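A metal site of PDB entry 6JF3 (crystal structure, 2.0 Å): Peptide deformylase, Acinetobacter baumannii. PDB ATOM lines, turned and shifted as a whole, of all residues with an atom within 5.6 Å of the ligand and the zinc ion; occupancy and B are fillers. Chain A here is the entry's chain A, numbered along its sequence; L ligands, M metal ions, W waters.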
ATOM      1  N   ARG A  45      26.568  -9.183 -22.048  1.00  0.00           N
ATOM      2  CA  ARG A  45      26.249  -8.657 -20.711  1.00  0.00           C
ATOM      3  C   ARG A  45      26.025  -9.780 -19.690  1.00  0.00           C
ATOM      4  O   ARG A  45      25.573  -9.508 -18.565  1.00  0.00           O
ATOM      5  CB  ARG A  45      25.018  -7.758 -20.744  1.00  0.00           C
ATOM      6  CG  ARG A  45      25.143  -6.519 -21.647  1.00  0.00           C
ATOM      7  CD  ARG A  45      25.663  -5.259 -20.951  1.00  0.00           C
ATOM      8  NE  ARG A  45      24.876  -4.858 -19.762  1.00  0.00           N
ATOM      9  CZ  ARG A  45      24.625  -3.600 -19.367  1.00  0.00           C
ATOM     10  NH1 ARG A  45      23.903  -3.404 -18.263  1.00  0.00           N
ATOM     11  NH2 ARG A  45      25.078  -2.551 -20.033  1.00  0.00           N
ATOM     12  N   ASN A  46      26.307 -11.026 -20.048  1.00  0.00           N
ATOM     13  CA  ASN A  46      26.054 -12.157 -19.131  1.00  0.00           C
ATOM     14  C   ASN A  46      24.630 -12.241 -18.574  1.00  0.00           C
ATOM     15  O   ASN A  46      24.402 -12.596 -17.419  1.00  0.00           O
ATOM     16  CB  ASN A  46      27.115 -12.176 -18.016  1.00  0.00           C
ATOM     17  CG  ASN A  46      28.119 -13.256 -18.233  1.00  0.00           C
ATOM     18  OD1 ASN A  46      27.865 -14.415 -17.907  1.00  0.00           O
ATOM     19  ND2 ASN A  46      29.258 -12.909 -18.815  1.00  0.00           N
ATOM     20  N   GLY A  47      23.651 -11.913 -19.404  1.00  0.00           N
ATOM     21  CA  GLY A  47      22.250 -12.104 -19.017  1.00  0.00           C
ATOM     22  C   GLY A  47      21.730 -13.463 -19.446  1.00  0.00           C
ATOM     23  O   GLY A  47      22.335 -14.151 -20.260  1.00  0.00           O
ATOM     24  N   VAL A  48      20.615 -13.850 -18.854  1.00  0.00           N
ATOM     25  CA  VAL A  48      19.967 -15.116 -19.156  1.00  0.00           C
ATOM     26  C   VAL A  48      18.663 -14.871 -19.914  1.00  0.00           C
ATOM     27  O   VAL A  48      17.950 -15.845 -20.247  1.00  0.00           O
ATOM     28  CB  VAL A  48      19.688 -15.929 -17.885  1.00  0.00           C
ATOM     29  CG1 VAL A  48      20.994 -16.429 -17.266  1.00  0.00           C
ATOM     30  CG2 VAL A  48      18.872 -15.124 -16.880  1.00  0.00           C
ATOM     31  N   GLY A  49      18.351 -13.576 -20.123  1.00  0.00           N
ATOM     32  CA  GLY A  49      17.363 -13.142 -21.100  1.00  0.00           C
ATOM     33  C   GLY A  49      17.484 -11.648 -21.430  1.00  0.00           C
ATOM     34  O   GLY A  49      18.312 -10.907 -20.816  1.00  0.00           O
ATOM     35  N   ILE A  50      16.627 -11.198 -22.348  1.00  0.00           N
ATOM     36  CA  ILE A  50      16.592  -9.794 -22.788  1.00  0.00           C
ATOM     37  C   ILE A  50      15.282  -9.450 -23.457  1.00  0.00           C
ATOM     38  O   ILE A  50      14.658 -10.294 -24.057  1.00  0.00           O
ATOM     39  CB  ILE A  50      17.793  -9.454 -23.707  1.00  0.00           C
ATOM     40  CG1 ILE A  50      17.953  -7.945 -23.898  1.00  0.00           C
ATOM     41  CG2 ILE A  50      17.738 -10.146 -25.049  1.00  0.00           C
ATOM     42  CD1 ILE A  50      19.401  -7.573 -24.195  1.00  0.00           C
ATOM     43  N   ALA A  51      14.818  -8.213 -23.289  1.00  0.00           N
ATOM     44  CA  ALA A  51      13.636  -7.733 -23.965  1.00  0.00           C
ATOM     45  C   ALA A  51      14.010  -6.515 -24.855  1.00  0.00           C
ATOM     46  O   ALA A  51      14.862  -5.676 -24.513  1.00  0.00           O
ATOM     47  CB  ALA A  51      12.604  -7.388 -22.921  1.00  0.00           C
ATOM     48  N   GLN A  54      14.889  -2.917 -23.612  1.00  0.00           N
ATOM     49  CA  GLN A  54      16.158  -2.706 -23.001  1.00  0.00           C
ATOM     50  C   GLN A  54      17.210  -2.239 -23.963  1.00  0.00           C
ATOM     51  O   GLN A  54      18.158  -1.615 -23.551  1.00  0.00           O
ATOM     52  CB  GLN A  54      16.639  -3.993 -22.323  1.00  0.00           C
ATOM     53  CG  GLN A  54      15.789  -4.412 -21.157  1.00  0.00           C
ATOM     54  CD  GLN A  54      16.291  -5.647 -20.487  1.00  0.00           C
ATOM     55  OE1 GLN A  54      16.070  -6.775 -21.005  1.00  0.00           O
ATOM     56  NE2 GLN A  54      16.957  -5.479 -19.329  1.00  0.00           N
ATOM     57  N   ARG A  67      20.954 -19.876 -18.341  1.00  0.00           N
ATOM     58  CA  ARG A  67      22.406 -20.111 -18.434  1.00  0.00           C
ATOM     59  C   ARG A  67      22.967 -20.145 -19.840  1.00  0.00           C
ATOM     60  O   ARG A  67      24.124 -19.777 -20.039  1.00  0.00           O
ATOM     61  CB  ARG A  67      22.788 -21.377 -17.706  1.00  0.00           C
ATOM     62  CG  ARG A  67      22.707 -21.273 -16.210  1.00  0.00           C
ATOM     63  CD  ARG A  67      23.873 -21.947 -15.533  1.00  0.00           C
ATOM     64  NE  ARG A  67      24.728 -20.911 -14.969  1.00  0.00           N
ATOM     65  CZ  ARG A  67      25.691 -20.254 -15.599  1.00  0.00           C
ATOM     66  NH1 ARG A  67      26.005 -20.496 -16.870  1.00  0.00           N
ATOM     67  NH2 ARG A  67      26.378 -19.325 -14.931  1.00  0.00           N
ATOM     68  N   ALA A  75      21.211 -22.317 -12.066  1.00  0.00           N
ATOM     69  CA  ALA A  75      20.179 -22.168 -13.119  1.00  0.00           C
ATOM     70  C   ALA A  75      20.227 -23.316 -14.143  1.00  0.00           C
ATOM     71  O   ALA A  75      21.315 -23.620 -14.656  1.00  0.00           O
ATOM     72  CB  ALA A  75      20.361 -20.821 -13.808  1.00  0.00           C
ATOM     73  N   GLU A  99      16.475 -14.652  -5.909  1.00  0.00           N
ATOM     74  CA  GLU A  99      17.125 -13.381  -6.222  1.00  0.00           C
ATOM     75  C   GLU A  99      17.134 -13.077  -7.749  1.00  0.00           C
ATOM     76  O   GLU A  99      17.606 -13.903  -8.543  1.00  0.00           O
ATOM     77  CB  GLU A  99      18.546 -13.287  -5.665  1.00  0.00           C
ATOM     78  CG  GLU A  99      19.152 -11.903  -5.871  1.00  0.00           C
ATOM     79  CD  GLU A  99      20.413 -11.682  -5.079  1.00  0.00           C
ATOM     80  OE1 GLU A  99      20.519 -10.619  -4.438  1.00  0.00           O
ATOM     81  OE2 GLU A  99      21.292 -12.565  -5.104  1.00  0.00           O
ATOM     82  N   GLU A 100      16.599 -11.906  -8.137  1.00  0.00           N
ATOM     83  CA  GLU A 100      16.602 -11.402  -9.536  1.00  0.00           C
ATOM     84  C   GLU A 100      17.449 -10.124  -9.615  1.00  0.00           C
ATOM     85  O   GLU A 100      17.449  -9.311  -8.710  1.00  0.00           O
ATOM     86  CB  GLU A 100      15.172 -11.077 -10.053  1.00  0.00           C
ATOM     87  CG  GLU A 100      14.198 -12.265 -10.061  1.00  0.00           C
ATOM     88  CD  GLU A 100      12.988 -12.115 -11.004  1.00  0.00           C
ATOM     89  OE1 GLU A 100      12.771 -11.051 -11.642  1.00  0.00           O
ATOM     90  OE2 GLU A 100      12.209 -13.082 -11.117  1.00  0.00           O
ATOM     91  N   GLY A 101      18.175  -9.981 -10.719  1.00  0.00           N
ATOM     92  CA  GLY A 101      18.814  -8.725 -11.100  1.00  0.00           C
ATOM     93  C   GLY A 101      18.476  -8.510 -12.556  1.00  0.00           C
ATOM     94  O   GLY A 101      17.981  -9.398 -13.207  1.00  0.00           O
ATOM     95  N   CYS A 102      18.770  -7.310 -13.043  1.00  0.00           N
ATOM     96  CA  CYS A 102      18.366  -6.855 -14.365  1.00  0.00           C
ATOM     97  C   CYS A 102      19.541  -6.074 -14.972  1.00  0.00           C
ATOM     98  O   CYS A 102      20.199  -5.278 -14.275  1.00  0.00           O
ATOM     99  CB  CYS A 102      17.136  -5.973 -14.194  1.00  0.00           C
ATOM    100  SG  CYS A 102      16.419  -5.262 -15.682  1.00  0.00           S
ATOM    101  N   LEU A 103      19.807  -6.324 -16.262  1.00  0.00           N
ATOM    102  CA  LEU A 103      20.848  -5.577 -17.016  1.00  0.00           C
ATOM    103  C   LEU A 103      20.569  -4.047 -16.986  1.00  0.00           C
ATOM    104  O   LEU A 103      21.506  -3.242 -17.236  1.00  0.00           O
ATOM    105  CB  LEU A 103      20.944  -6.008 -18.505  1.00  0.00           C
ATOM    106  CG  LEU A 103      21.200  -7.480 -18.877  1.00  0.00           C
ATOM    107  CD1 LEU A 103      21.048  -7.700 -20.394  1.00  0.00           C
ATOM    108  CD2 LEU A 103      22.557  -7.962 -18.335  1.00  0.00           C
ATOM    109  N   SER A 104      19.301  -3.683 -16.728  1.00  0.00           N
ATOM    110  CA  SER A 104      18.825  -2.303 -16.711  1.00  0.00           C
ATOM    111  C   SER A 104      18.702  -1.652 -15.304  1.00  0.00           C
ATOM    112  O   SER A 104      18.079  -0.572 -15.198  1.00  0.00           O
ATOM    113  CB  SER A 104      17.453  -2.239 -17.438  1.00  0.00           C
ATOM    114  OG  SER A 104      17.603  -2.694 -18.781  1.00  0.00           O
ATOM    115  N   ARG A 109      19.427  -5.527  -7.084  1.00  0.00           N
ATOM    116  CA  ARG A 109      18.904  -6.901  -6.929  1.00  0.00           C
ATOM    117  C   ARG A 109      17.950  -7.098  -5.713  1.00  0.00           C
ATOM    118  O   ARG A 109      17.725  -6.164  -4.941  1.00  0.00           O
ATOM    119  CB  ARG A 109      20.069  -7.921  -6.909  1.00  0.00           C
ATOM    120  CG  ARG A 109      21.222  -7.536  -7.824  1.00  0.00           C
ATOM    121  CD  ARG A 109      21.858  -8.723  -8.560  1.00  0.00           C
ATOM    122  NE  ARG A 109      22.415  -9.742  -7.682  1.00  0.00           N
ATOM    123  CZ  ARG A 109      23.517  -9.616  -6.934  1.00  0.00           C
ATOM    124  NH1 ARG A 109      23.940 -10.642  -6.198  1.00  0.00           N
ATOM    125  NH2 ARG A 109      24.209  -8.470  -6.900  1.00  0.00           N
ATOM    126  N   ARG A 114       7.512 -15.266  -8.172  1.00  0.00           N
ATOM    127  CA  ARG A 114       7.033 -15.546  -9.545  1.00  0.00           C
ATOM    128  C   ARG A 114       6.158 -16.792  -9.585  1.00  0.00           C
ATOM    129  O   ARG A 114       6.328 -17.695  -8.749  1.00  0.00           O
ATOM    130  CB  ARG A 114       8.234 -15.786 -10.448  1.00  0.00           C
ATOM    131  CG  ARG A 114       9.198 -14.620 -10.632  1.00  0.00           C
ATOM    132  CD  ARG A 114       8.518 -13.477 -11.352  1.00  0.00           C
ATOM    133  NE  ARG A 114       9.490 -12.461 -11.739  1.00  0.00           N
ATOM    134  CZ  ARG A 114       9.214 -11.293 -12.290  1.00  0.00           C
ATOM    135  NH1 ARG A 114       7.972 -10.926 -12.564  1.00  0.00           N
ATOM    136  NH2 ARG A 114      10.251 -10.479 -12.548  1.00  0.00           N
ATOM    137  N   PHE A 137      13.128 -21.669 -13.011  1.00  0.00           N
ATOM    138  CA  PHE A 137      13.858 -20.462 -13.397  1.00  0.00           C
ATOM    139  C   PHE A 137      13.559 -19.913 -14.801  1.00  0.00           C
ATOM    140  O   PHE A 137      13.268 -18.742 -14.938  1.00  0.00           O
ATOM    141  CB  PHE A 137      15.347 -20.657 -13.180  1.00  0.00           C
ATOM    142  CG  PHE A 137      16.137 -19.376 -13.250  1.00  0.00           C
ATOM    143  CD1 PHE A 137      15.820 -18.272 -12.423  1.00  0.00           C
ATOM    144  CD2 PHE A 137      17.248 -19.262 -14.123  1.00  0.00           C
ATOM    145  CE1 PHE A 137      16.585 -17.117 -12.469  1.00  0.00           C
ATOM    146  CE2 PHE A 137      18.006 -18.097 -14.177  1.00  0.00           C
ATOM    147  CZ  PHE A 137      17.666 -17.026 -13.357  1.00  0.00           C
ATOM    148  N   ARG A 140      10.508 -17.912 -14.566  1.00  0.00           N
ATOM    149  CA  ARG A 140      10.797 -16.606 -13.987  1.00  0.00           C
ATOM    150  C   ARG A 140      11.432 -15.660 -15.028  1.00  0.00           C
ATOM    151  O   ARG A 140      11.074 -14.496 -15.100  1.00  0.00           O
ATOM    152  CB  ARG A 140      11.711 -16.707 -12.757  1.00  0.00           C
ATOM    153  CG  ARG A 140      11.023 -17.353 -11.596  1.00  0.00           C
ATOM    154  N   ILE A 141      12.359 -16.178 -15.841  1.00  0.00           N
ATOM    155  CA  ILE A 141      12.955 -15.398 -16.869  1.00  0.00           C
ATOM    156  C   ILE A 141      11.860 -14.889 -17.813  1.00  0.00           C
ATOM    157  O   ILE A 141      11.845 -13.717 -18.099  1.00  0.00           O
ATOM    158  CB  ILE A 141      14.057 -16.136 -17.689  1.00  0.00           C
ATOM    159  CG1 ILE A 141      15.217 -16.598 -16.790  1.00  0.00           C
ATOM    160  CG2 ILE A 141      14.634 -15.168 -18.711  1.00  0.00           C
ATOM    161  CD1 ILE A 141      16.168 -17.602 -17.434  1.00  0.00           C
ATOM    162  N   HIS A 144       9.780 -12.083 -16.123  1.00  0.00           N
ATOM    163  CA  HIS A 144      10.572 -10.903 -16.116  1.00  0.00           C
ATOM    164  C   HIS A 144      10.643 -10.162 -17.460  1.00  0.00           C
ATOM    165  O   HIS A 144      10.549  -8.936 -17.500  1.00  0.00           O
ATOM    166  CB  HIS A 144      11.974 -11.286 -15.664  1.00  0.00           C
ATOM    167  CG  HIS A 144      12.898 -10.147 -15.531  1.00  0.00           C
ATOM    168  ND1 HIS A 144      13.256  -9.618 -14.324  1.00  0.00           N
ATOM    169  CD2 HIS A 144      13.580  -9.454 -16.473  1.00  0.00           C
ATOM    170  CE1 HIS A 144      14.129  -8.646 -14.510  1.00  0.00           C
ATOM    171  NE2 HIS A 144      14.331  -8.523 -15.804  1.00  0.00           N
ATOM    172  N   GLU A 145      10.856 -10.900 -18.549  1.00  0.00           N
ATOM    173  CA  GLU A 145      11.016 -10.252 -19.852  1.00  0.00           C
ATOM    174  C   GLU A 145       9.663  -9.686 -20.341  1.00  0.00           C
ATOM    175  O   GLU A 145       9.590  -8.543 -20.836  1.00  0.00           O
ATOM    176  CB  GLU A 145      11.585 -11.227 -20.892  1.00  0.00           C
ATOM    177  CG  GLU A 145      12.947 -11.838 -20.597  1.00  0.00           C
ATOM    178  CD  GLU A 145      13.978 -10.844 -20.188  1.00  0.00           C
ATOM    179  OE1 GLU A 145      13.810  -9.671 -20.614  1.00  0.00           O
ATOM    180  OE2 GLU A 145      14.955 -11.231 -19.467  1.00  0.00           O
ATOM    181  N   HIS A 148       9.086  -6.484 -18.786  1.00  0.00           N
ATOM    182  CA  HIS A 148       9.704  -5.434 -19.527  1.00  0.00           C
ATOM    183  C   HIS A 148       8.841  -4.920 -20.674  1.00  0.00           C
ATOM    184  O   HIS A 148       8.767  -3.717 -20.871  1.00  0.00           O
ATOM    185  CB  HIS A 148      11.054  -5.805 -20.053  1.00  0.00           C
ATOM    186  CG  HIS A 148      12.148  -5.725 -19.055  1.00  0.00           C
ATOM    187  ND1 HIS A 148      12.521  -4.537 -18.456  1.00  0.00           N
ATOM    188  CD2 HIS A 148      13.015  -6.666 -18.607  1.00  0.00           C
ATOM    189  CE1 HIS A 148      13.557  -4.756 -17.656  1.00  0.00           C
ATOM    190  NE2 HIS A 148      13.865  -6.045 -17.706  1.00  0.00           N
HETATM  191  C1  LIG L   1      18.662  -9.907 -17.593  1.00  0.00           C
HETATM  192  C2  LIG L   1      17.601  -8.882 -17.910  1.00  0.00           C
HETATM  193  O1  LIG L   1      17.606  -7.805 -17.342  1.00  0.00           O
HETATM  194  N1  LIG L   1      16.654  -9.271 -18.780  1.00  0.00           N
HETATM  195  O2  LIG L   1      15.518  -8.501 -19.012  1.00  0.00           O
HETATM  196  C3  LIG L   1      18.356 -10.573 -16.249  1.00  0.00           C
HETATM  197  C4  LIG L   1      19.604 -11.282 -15.882  1.00  0.00           C
HETATM  198  O3  LIG L   1      20.180 -11.915 -16.744  1.00  0.00           O
HETATM  199  C5  LIG L   1      17.205 -11.596 -16.296  1.00  0.00           C
HETATM  200  C6  LIG L   1      16.751 -11.963 -14.867  1.00  0.00           C
HETATM  201  C7  LIG L   1      15.718 -13.081 -14.801  1.00  0.00           C
HETATM  202  C8  LIG L   1      15.556 -13.564 -13.367  1.00  0.00           C
HETATM  203  C9  LIG L   1      14.267 -14.329 -13.195  1.00  0.00           C
HETATM  204  N2  LIG L   1      19.987 -11.230 -14.603  1.00  0.00           N
HETATM  205  C10 LIG L   1      21.093 -12.069 -14.096  1.00  0.00           C
HETATM  206  C11 LIG L   1      22.295 -11.170 -13.753  1.00  0.00           C
HETATM  207  C12 LIG L   1      22.661 -10.294 -14.974  1.00  0.00           C
HETATM  208  C13 LIG L   1      22.071 -10.357 -12.481  1.00  0.00           C
HETATM  209  C14 LIG L   1      20.593 -13.017 -12.982  1.00  0.00           C
HETATM  210  O4  LIG L   1      19.700 -12.647 -12.204  1.00  0.00           O
HETATM  211  N3  LIG L   1      21.147 -14.279 -12.930  1.00  0.00           N
HETATM  212  C15 LIG L   1      20.661 -15.299 -11.974  1.00  0.00           C
HETATM  213  C16 LIG L   1      22.243 -14.818 -13.774  1.00  0.00           C
HETATM  214  C17 LIG L   1      22.421 -16.269 -13.365  1.00  0.00           C
HETATM  215  C18 LIG L   1      21.230 -16.625 -12.482  1.00  0.00           C
HETATM  216  C19 LIG L   1      21.153 -14.957 -10.556  1.00  0.00           C
HETATM  217  O5  LIG L   1      20.083 -14.427  -9.788  1.00  0.00           O
HETATM  218 ZN    ZN M   1      15.595  -7.148 -16.887  1.00  0.00          ZN
HETATM  219  O   HOH W   1      13.614  -5.689 -14.580  1.00  0.00           O
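Merely in contact with the zinc ion: Gln 54 (3.3 Å).
The zinc ion is bound by a ring nitrogen (NE2) of His 144 (2.2 Å), an oxygen (O1) of the ligand (2.2 Å), a ring nitrogen (NE2) of His 148 (2.2 Å), the side-chain sulfur (SG) of Cys 102 (2.4 Å) and an oxygen (O2) of the ligand (2.5 Å).
O of Asn 46 touches C12 of the ligand, at 3.8 Å.
Gly 47 touches the ligand.
OE2 of Glu 100 touches C9 of the ligand, 3.2 Å away.
Phe 137 touches the ligand (CZ to C18, 3.7 Å).
Arg 140 touches the ligand (CB to C9, 3.5 Å).
N of Ile 141 touches C9 of the ligand, 3.7 Å away.
Hydrophobic or aromatic side chains within 4 Å of the ligand: Val 48, Leu 103, Phe 137, His 144 and His 148.
Along chain A the residues within 4 Å of the ligand span positions 46 to 148.
The nearest printed residue that does not touch the ligand is Ile 50 (4.04 Å).
ND1 of His 144 is in hydrogen-bond range of OE1 of Glu 100, at 3.1 Å.
The side-chain sulfur (SG) of Cys 102 lies close to the backbone NH (N) of Ser 104 (3.4 Å).
The backbone NH (N) of Ala 51 is in hydrogen-bond range of the side-chain carboxylate (OE1) of Glu 145 (3.2 Å).
The backbone NH (N) of Ala 51 sits at hydrogen-bond distance from the side-chain amide oxygen (OE1) of Gln 54.
OG of Ser 104 sits at hydrogen-bond distance from NE2 of Gln 54.
OE2 of Glu 99 lies within salt-bridge range of NH1 of Arg 109 (3.5 Å).
O of Leu 103 lies within hydrogen-bond range of NH1 of Arg 45 (2.6 Å).
The guanidinium group of Arg 114 lies within salt-bridge range of the side-chain carboxylate of Glu 100, at 2.7 Å.
N1 of the ligand sits at hydrogen-bond distance from OE2 of Glu 145.
A nitrogen (N1) of the ligand lies within hydrogen-bond range of the side-chain amide oxygen (OE1) of Gln 54.
O5 of the ligand sits at hydrogen-bond distance from O of Glu 99, at 2.8 Å.
The backbone NH (N) of Leu 103 lies close to an oxygen (O1) of the ligand, at 2.9 Å.
The backbone NH (N) of Val 48 sits at hydrogen-bond distance from an oxygen (O3) of the ligand, at 2.9 Å.
The backbone NH (N) of Gly 101 is in hydrogen-bond range of an oxygen (O4) of the ligand (3.4 Å).
The backbone carbonyl oxygen (O) of Gly 101 is in hydrogen-bond range of a nitrogen (N2) of the ligand, at 3.1 Å.
The backbone carbonyl oxygen (O) of Gly 49 lies within hydrogen-bond range of a nitrogen (N1) of the ligand, 3.1 Å away.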
